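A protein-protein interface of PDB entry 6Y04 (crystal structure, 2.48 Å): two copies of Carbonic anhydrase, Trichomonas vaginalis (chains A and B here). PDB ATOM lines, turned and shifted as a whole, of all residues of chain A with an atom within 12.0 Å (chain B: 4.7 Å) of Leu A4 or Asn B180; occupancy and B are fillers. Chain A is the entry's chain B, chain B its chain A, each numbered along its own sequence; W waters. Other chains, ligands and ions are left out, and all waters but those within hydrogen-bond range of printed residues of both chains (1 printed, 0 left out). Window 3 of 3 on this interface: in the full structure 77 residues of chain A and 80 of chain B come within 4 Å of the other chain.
OH of Tyr B182 sits at hydrogen-bond distance from N of Gln A3, 3.3 Å away. N of Leu A4 is in hydrogen-bond range of OH of Tyr B182 (3.3 Å).
The side-chain amide oxygen (OD1) of Asn B180 is in hydrogen-bond range of the backbone NH (N) of Tyr B182. OG of Ser A2 sits close to N of Leu A4, at 3.4 Å. N of Ser A2 sits at hydrogen-bond distance from OE1 of Glu A5, at 2.9 Å. The side-chain hydroxyl (OG1) of Thr A8 sits at hydrogen-bond distance from the backbone carbonyl oxygen (O) of Leu A4, 3.0 Å away.
Among the printed residues, pairs that only touch across the chains: Leu A4 with Asn B180, Ser A2 with Tyr B182, Ile A7 with Phe B92, Leu A4 with Leu B166, Gln A3 with Phe B92, Leu A4 with Thr B177 and Leu A4 with Phe B92.
Of the printed residues of chain B, Gln A3 touches Phe B92 and Tyr B182. Leu A4 touches just these residues of chain B: Phe B92 (3.97 Å), Leu B166 (3.8 Å), Thr B177 (3.96 Å), Asn B180 (3.4 Å) and Tyr B182 (3.3 Å). Leu A6 touches none of the printed residues of chain B. Of the printed residues of chain B, Ile A7 touches Phe B92 (3.6 Å). Asn A11 touches none of the printed residues of chain B. Of the printed residues of chain A, Phe B92 touches Gln A3, Leu A4 and Ile A7. No residue of chain A comes within 4 Å of His B164. Of the printed residues of chain A, Leu B166 touches Leu A4. Of chain A, only Leu A4 comes within 4 Å of Thr B177. Ile B179 touches none of the printed residues of chain A. Of chain A, only Leu A4 (3.4 Å) comes within 4 Å of Asn B180. Of chain A, only Ser A2 (3.5 Å), Gln A3 (3.3 Å) and Leu A4 (3.3 Å) come within 4 Å of Tyr B182. The nearest printed residue of chain B that does not touch Gln A3 is His B164 (6.0 Å).
Of the 9 printed residues of chain B, 5 touch a printed residue of chain A. Hydrophobic or aromatic side chains of chain B within 4 Å of the printed part of chain A: Phe B92, Leu B166 and Tyr B182. Among the printed residues, no Asp or Glu carboxylate lies within 4 Å of a Lys or Arg side-chain nitrogen of the other chain.
No position is printed for both chains. Of the 9 pairs that touch across the chains among the printed residues, none has its exchanged pair printed and touching as well.
Water W1 bridges the backbone NH (N) of Gln A3 and the side-chain hydroxyl (OH) of Tyr B182.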
ATOM      1  N   MET A   1     -16.419  31.174  -3.915  1.00  0.00           N
ATOM      2  CA  MET A   1     -15.495  31.041  -2.726  1.00  0.00           C
ATOM      3  C   MET A   1     -15.856  29.815  -1.894  1.00  0.00           C
ATOM      4  O   MET A   1     -17.006  29.642  -1.509  1.00  0.00           O
ATOM      5  CB  MET A   1     -15.560  32.255  -1.795  1.00  0.00           C
ATOM      6  CG  MET A   1     -14.904  33.491  -2.333  1.00  0.00           C
ATOM      7  SD  MET A   1     -13.822  34.162  -1.057  1.00  0.00           S
ATOM      8  CE  MET A   1     -12.230  33.798  -1.796  1.00  0.00           C
ATOM      9  N   SER A   2     -14.850  28.985  -1.600  1.00  0.00           N
ATOM     10  CA  SER A   2     -15.031  27.794  -0.782  1.00  0.00           C
ATOM     11  C   SER A   2     -15.083  28.170   0.700  1.00  0.00           C
ATOM     12  O   SER A   2     -14.720  29.289   1.082  1.00  0.00           O
ATOM     13  CB  SER A   2     -13.936  26.793  -1.052  1.00  0.00           C
ATOM     14  OG  SER A   2     -12.792  27.082  -0.269  1.00  0.00           O
ATOM     15  N   GLN A   3     -15.508  27.209   1.532  1.00  0.00           N
ATOM     16  CA  GLN A   3     -15.663  27.440   2.962  1.00  0.00           C
ATOM     17  C   GLN A   3     -14.302  27.712   3.595  1.00  0.00           C
ATOM     18  O   GLN A   3     -14.193  28.526   4.508  1.00  0.00           O
ATOM     19  CB  GLN A   3     -16.376  26.268   3.637  1.00  0.00           C
ATOM     20  CG  GLN A   3     -17.850  26.149   3.269  1.00  0.00           C
ATOM     21  CD  GLN A   3     -18.660  27.341   3.710  1.00  0.00           C
ATOM     22  OE1 GLN A   3     -18.524  27.831   4.834  1.00  0.00           O
ATOM     23  NE2 GLN A   3     -19.504  27.833   2.811  1.00  0.00           N
ATOM     24  N   LEU A   4     -13.271  27.029   3.088  1.00  0.00           N
ATOM     25  CA  LEU A   4     -11.910  27.224   3.556  1.00  0.00           C
ATOM     26  C   LEU A   4     -11.460  28.644   3.224  1.00  0.00           C
ATOM     27  O   LEU A   4     -10.872  29.323   4.071  1.00  0.00           O
ATOM     28  CB  LEU A   4     -10.995  26.169   2.923  1.00  0.00           C
ATOM     29  CG  LEU A   4      -9.523  26.241   3.333  1.00  0.00           C
ATOM     30  CD1 LEU A   4      -9.360  26.034   4.824  1.00  0.00           C
ATOM     31  CD2 LEU A   4      -8.686  25.224   2.572  1.00  0.00           C
ATOM     32  N   GLU A   5     -11.770  29.088   1.999  1.00  0.00           N
ATOM     33  CA  GLU A   5     -11.370  30.410   1.547  1.00  0.00           C
ATOM     34  C   GLU A   5     -12.033  31.470   2.421  1.00  0.00           C
ATOM     35  O   GLU A   5     -11.406  32.472   2.748  1.00  0.00           O
ATOM     36  CB  GLU A   5     -11.691  30.616   0.065  1.00  0.00           C
ATOM     37  CG  GLU A   5     -10.823  29.766  -0.846  1.00  0.00           C
ATOM     38  CD  GLU A   5     -11.128  29.782  -2.337  1.00  0.00           C
ATOM     39  OE1 GLU A   5     -12.325  29.765  -2.728  1.00  0.00           O
ATOM     40  OE2 GLU A   5     -10.169  29.784  -3.110  1.00  0.00           O
ATOM     41  N   LEU A   6     -13.296  31.228   2.791  1.00  0.00           N
ATOM     42  CA  LEU A   6     -14.078  32.156   3.594  1.00  0.00           C
ATOM     43  C   LEU A   6     -13.479  32.272   4.993  1.00  0.00           C
ATOM     44  O   LEU A   6     -13.424  33.366   5.549  1.00  0.00           O
ATOM     45  CB  LEU A   6     -15.535  31.685   3.647  1.00  0.00           C
ATOM     46  CG  LEU A   6     -16.366  31.960   2.386  1.00  0.00           C
ATOM     47  CD1 LEU A   6     -17.769  31.388   2.518  1.00  0.00           C
ATOM     48  CD2 LEU A   6     -16.415  33.449   2.025  1.00  0.00           C
ATOM     49  N   ILE A   7     -13.023  31.138   5.545  1.00  0.00           N
ATOM     50  CA  ILE A   7     -12.366  31.097   6.845  1.00  0.00           C
ATOM     51  C   ILE A   7     -11.037  31.855   6.777  1.00  0.00           C
ATOM     52  O   ILE A   7     -10.770  32.686   7.642  1.00  0.00           O
ATOM     53  CB  ILE A   7     -12.232  29.646   7.365  1.00  0.00           C
ATOM     54  CG1 ILE A   7     -13.531  29.167   8.019  1.00  0.00           C
ATOM     55  CG2 ILE A   7     -11.051  29.499   8.315  1.00  0.00           C
ATOM     56  CD1 ILE A   7     -13.738  27.663   7.990  1.00  0.00           C
ATOM     57  N   THR A   8     -10.231  31.589   5.736  1.00  0.00           N
ATOM     58  CA  THR A   8      -8.959  32.260   5.509  1.00  0.00           C
ATOM     59  C   THR A   8      -9.175  33.769   5.470  1.00  0.00           C
ATOM     60  O   THR A   8      -8.465  34.533   6.120  1.00  0.00           O
ATOM     61  CB  THR A   8      -8.339  31.833   4.173  1.00  0.00           C
ATOM     62  OG1 THR A   8      -8.102  30.428   4.243  1.00  0.00           O
ATOM     63  CG2 THR A   8      -7.044  32.547   3.847  1.00  0.00           C
ATOM     64  N   SER A   9     -10.169  34.165   4.678  1.00  0.00           N
ATOM     65  CA  SER A   9     -10.576  35.542   4.474  1.00  0.00           C
ATOM     66  C   SER A   9     -11.008  36.183   5.799  1.00  0.00           C
ATOM     67  O   SER A   9     -10.537  37.260   6.164  1.00  0.00           O
ATOM     68  CB  SER A   9     -11.662  35.563   3.423  1.00  0.00           C
ATOM     69  OG  SER A   9     -12.170  36.869   3.210  1.00  0.00           O
ATOM     70  N   ALA A  10     -11.888  35.499   6.543  1.00  0.00           N
ATOM     71  CA  ALA A  10     -12.406  36.034   7.793  1.00  0.00           C
ATOM     72  C   ALA A  10     -11.276  36.203   8.809  1.00  0.00           C
ATOM     73  O   ALA A  10     -11.287  37.142   9.606  1.00  0.00           O
ATOM     74  CB  ALA A  10     -13.493  35.139   8.321  1.00  0.00           C
ATOM     75  N   ASN A  11     -10.299  35.287   8.762  1.00  0.00           N
ATOM     76  CA  ASN A  11      -9.186  35.315   9.697  1.00  0.00           C
ATOM     77  C   ASN A  11      -8.328  36.547   9.444  1.00  0.00           C
ATOM     78  O   ASN A  11      -7.883  37.192  10.387  1.00  0.00           O
ATOM     79  CB  ASN A  11      -8.323  34.054   9.635  1.00  0.00           C
ATOM     80  CG  ASN A  11      -7.238  34.042  10.693  1.00  0.00           C
ATOM     81  OD1 ASN A  11      -6.050  34.029  10.367  1.00  0.00           O
ATOM     82  ND2 ASN A  11      -7.634  34.046  11.960  1.00  0.00           N
ATOM     83  N   GLN A  12      -8.101  36.847   8.159  1.00  0.00           N
ATOM     84  CA  GLN A  12      -7.325  38.009   7.762  1.00  0.00           C
ATOM     85  C   GLN A  12      -7.966  39.255   8.366  1.00  0.00           C
ATOM     86  O   GLN A  12      -7.288  40.036   9.029  1.00  0.00           O
ATOM     87  CB  GLN A  12      -7.203  38.072   6.234  1.00  0.00           C
ATOM     88  CG  GLN A  12      -6.204  39.108   5.737  1.00  0.00           C
ATOM     89  CD  GLN A  12      -5.878  38.989   4.264  1.00  0.00           C
ATOM     90  OE1 GLN A  12      -5.650  37.907   3.723  1.00  0.00           O
ATOM     91  NE2 GLN A  12      -5.835  40.130   3.597  1.00  0.00           N
ATOM     92  N   ALA A  13      -9.285  39.392   8.168  1.00  0.00           N
ATOM     93  CA  ALA A  13     -10.064  40.511   8.681  1.00  0.00           C
ATOM     94  C   ALA A  13     -10.041  40.536  10.209  1.00  0.00           C
ATOM     95  O   ALA A  13     -10.069  41.608  10.813  1.00  0.00           O
ATOM     96  CB  ALA A  13     -11.474  40.441   8.154  1.00  0.00           C
ATOM     97  N   PHE B  92     -13.669  20.593   9.574  1.00  0.00           N
ATOM     98  CA  PHE B  92     -12.414  21.273   9.844  1.00  0.00           C
ATOM     99  C   PHE B  92     -11.873  20.819  11.195  1.00  0.00           C
ATOM    100  O   PHE B  92     -12.536  20.989  12.221  1.00  0.00           O
ATOM    101  CB  PHE B  92     -12.633  22.785   9.875  1.00  0.00           C
ATOM    102  CG  PHE B  92     -13.095  23.370   8.567  1.00  0.00           C
ATOM    103  CD1 PHE B  92     -14.418  23.245   8.163  1.00  0.00           C
ATOM    104  CD2 PHE B  92     -12.205  24.035   7.735  1.00  0.00           C
ATOM    105  CE1 PHE B  92     -14.846  23.773   6.952  1.00  0.00           C
ATOM    106  CE2 PHE B  92     -12.633  24.563   6.525  1.00  0.00           C
ATOM    107  CZ  PHE B  92     -13.950  24.435   6.138  1.00  0.00           C
ATOM    108  N   HIS B 164     -10.489  19.031   6.436  1.00  0.00           N
ATOM    109  CA  HIS B 164      -9.429  20.028   6.422  1.00  0.00           C
ATOM    110  C   HIS B 164      -8.697  20.046   7.761  1.00  0.00           C
ATOM    111  O   HIS B 164      -9.239  19.652   8.788  1.00  0.00           O
ATOM    112  CB  HIS B 164      -9.983  21.425   6.105  1.00  0.00           C
ATOM    113  CG  HIS B 164     -11.021  21.443   5.039  1.00  0.00           C
ATOM    114  ND1 HIS B 164     -10.700  21.469   3.708  1.00  0.00           N
ATOM    115  CD2 HIS B 164     -12.369  21.440   5.105  1.00  0.00           C
ATOM    116  CE1 HIS B 164     -11.807  21.479   2.992  1.00  0.00           C
ATOM    117  NE2 HIS B 164     -12.847  21.456   3.827  1.00  0.00           N
ATOM    118  N   LEU B 166      -6.446  22.737  10.218  1.00  0.00           N
ATOM    119  CA  LEU B 166      -6.069  24.113  10.495  1.00  0.00           C
ATOM    120  C   LEU B 166      -5.262  24.166  11.787  1.00  0.00           C
ATOM    121  O   LEU B 166      -5.393  23.305  12.658  1.00  0.00           O
ATOM    122  CB  LEU B 166      -7.327  24.974  10.622  1.00  0.00           C
ATOM    123  CG  LEU B 166      -8.279  24.952   9.427  1.00  0.00           C
ATOM    124  CD1 LEU B 166      -9.486  25.837   9.687  1.00  0.00           C
ATOM    125  CD2 LEU B 166      -7.580  25.379   8.145  1.00  0.00           C
ATOM    126  N   THR B 177      -3.625  27.236   7.272  1.00  0.00           N
ATOM    127  CA  THR B 177      -4.074  26.001   6.653  1.00  0.00           C
ATOM    128  C   THR B 177      -2.950  24.969   6.698  1.00  0.00           C
ATOM    129  O   THR B 177      -1.811  25.270   6.356  1.00  0.00           O
ATOM    130  CB  THR B 177      -4.559  26.281   5.225  1.00  0.00           C
ATOM    131  OG1 THR B 177      -5.619  27.227   5.353  1.00  0.00           O
ATOM    132  CG2 THR B 177      -5.064  25.066   4.481  1.00  0.00           C
ATOM    133  N   ILE B 178      -3.283  23.754   7.134  1.00  0.00           N
ATOM    134  CA  ILE B 178      -2.321  22.663   7.173  1.00  0.00           C
ATOM    135  C   ILE B 178      -2.675  21.653   6.083  1.00  0.00           C
ATOM    136  O   ILE B 178      -1.824  21.308   5.268  1.00  0.00           O
ATOM    137  CB  ILE B 178      -2.270  22.026   8.575  1.00  0.00           C
ATOM    138  CG1 ILE B 178      -2.034  23.065   9.677  1.00  0.00           C
ATOM    139  CG2 ILE B 178      -1.246  20.901   8.625  1.00  0.00           C
ATOM    140  CD1 ILE B 178      -0.719  23.823   9.580  1.00  0.00           C
ATOM    141  N   ILE B 179      -3.942  21.207   6.063  1.00  0.00           N
ATOM    142  CA  ILE B 179      -4.415  20.312   5.015  1.00  0.00           C
ATOM    143  C   ILE B 179      -5.673  20.885   4.370  1.00  0.00           C
ATOM    144  O   ILE B 179      -6.613  21.257   5.066  1.00  0.00           O
ATOM    145  CB  ILE B 179      -4.635  18.880   5.548  1.00  0.00           C
ATOM    146  CG1 ILE B 179      -3.310  18.226   5.944  1.00  0.00           C
ATOM    147  CG2 ILE B 179      -5.376  18.019   4.537  1.00  0.00           C
ATOM    148  CD1 ILE B 179      -3.464  16.908   6.681  1.00  0.00           C
ATOM    149  N   ASN B 180      -5.675  20.949   3.034  1.00  0.00           N
ATOM    150  CA  ASN B 180      -6.859  21.277   2.252  1.00  0.00           C
ATOM    151  C   ASN B 180      -7.482  19.969   1.765  1.00  0.00           C
ATOM    152  O   ASN B 180      -6.831  19.205   1.059  1.00  0.00           O
ATOM    153  CB  ASN B 180      -6.500  22.203   1.084  1.00  0.00           C
ATOM    154  CG  ASN B 180      -7.653  22.530   0.153  1.00  0.00           C
ATOM    155  OD1 ASN B 180      -8.491  21.679  -0.153  1.00  0.00           O
ATOM    156  ND2 ASN B 180      -7.702  23.768  -0.308  1.00  0.00           N
ATOM    157  N   GLY B 181      -8.748  19.723   2.133  1.00  0.00           N
ATOM    158  CA  GLY B 181      -9.324  18.397   1.980  1.00  0.00           C
ATOM    159  C   GLY B 181     -10.250  18.236   0.777  1.00  0.00           C
ATOM    160  O   GLY B 181     -10.923  17.217   0.683  1.00  0.00           O
ATOM    161  N   TYR B 182     -10.249  19.195  -0.162  1.00  0.00           N
ATOM    162  CA  TYR B 182     -11.248  19.213  -1.226  1.00  0.00           C
ATOM    163  C   TYR B 182     -11.025  18.098  -2.250  1.00  0.00           C
ATOM    164  O   TYR B 182      -9.908  18.082  -2.765  1.00  0.00           O
ATOM    165  CB  TYR B 182     -11.357  20.592  -1.875  1.00  0.00           C
ATOM    166  CG  TYR B 182     -12.095  21.572  -1.004  1.00  0.00           C
ATOM    167  CD1 TYR B 182     -13.349  21.269  -0.499  1.00  0.00           C
ATOM    168  CD2 TYR B 182     -11.520  22.782  -0.649  1.00  0.00           C
ATOM    169  CE1 TYR B 182     -14.016  22.151   0.337  1.00  0.00           C
ATOM    170  CE2 TYR B 182     -12.175  23.677   0.180  1.00  0.00           C
ATOM    171  CZ  TYR B 182     -13.426  23.359   0.682  1.00  0.00           C
ATOM    172  OH  TYR B 182     -14.064  24.237   1.509  1.00  0.00           O
HETATM  173  O   HOH W   1     -16.668  25.175   0.378  1.00  0.00           O
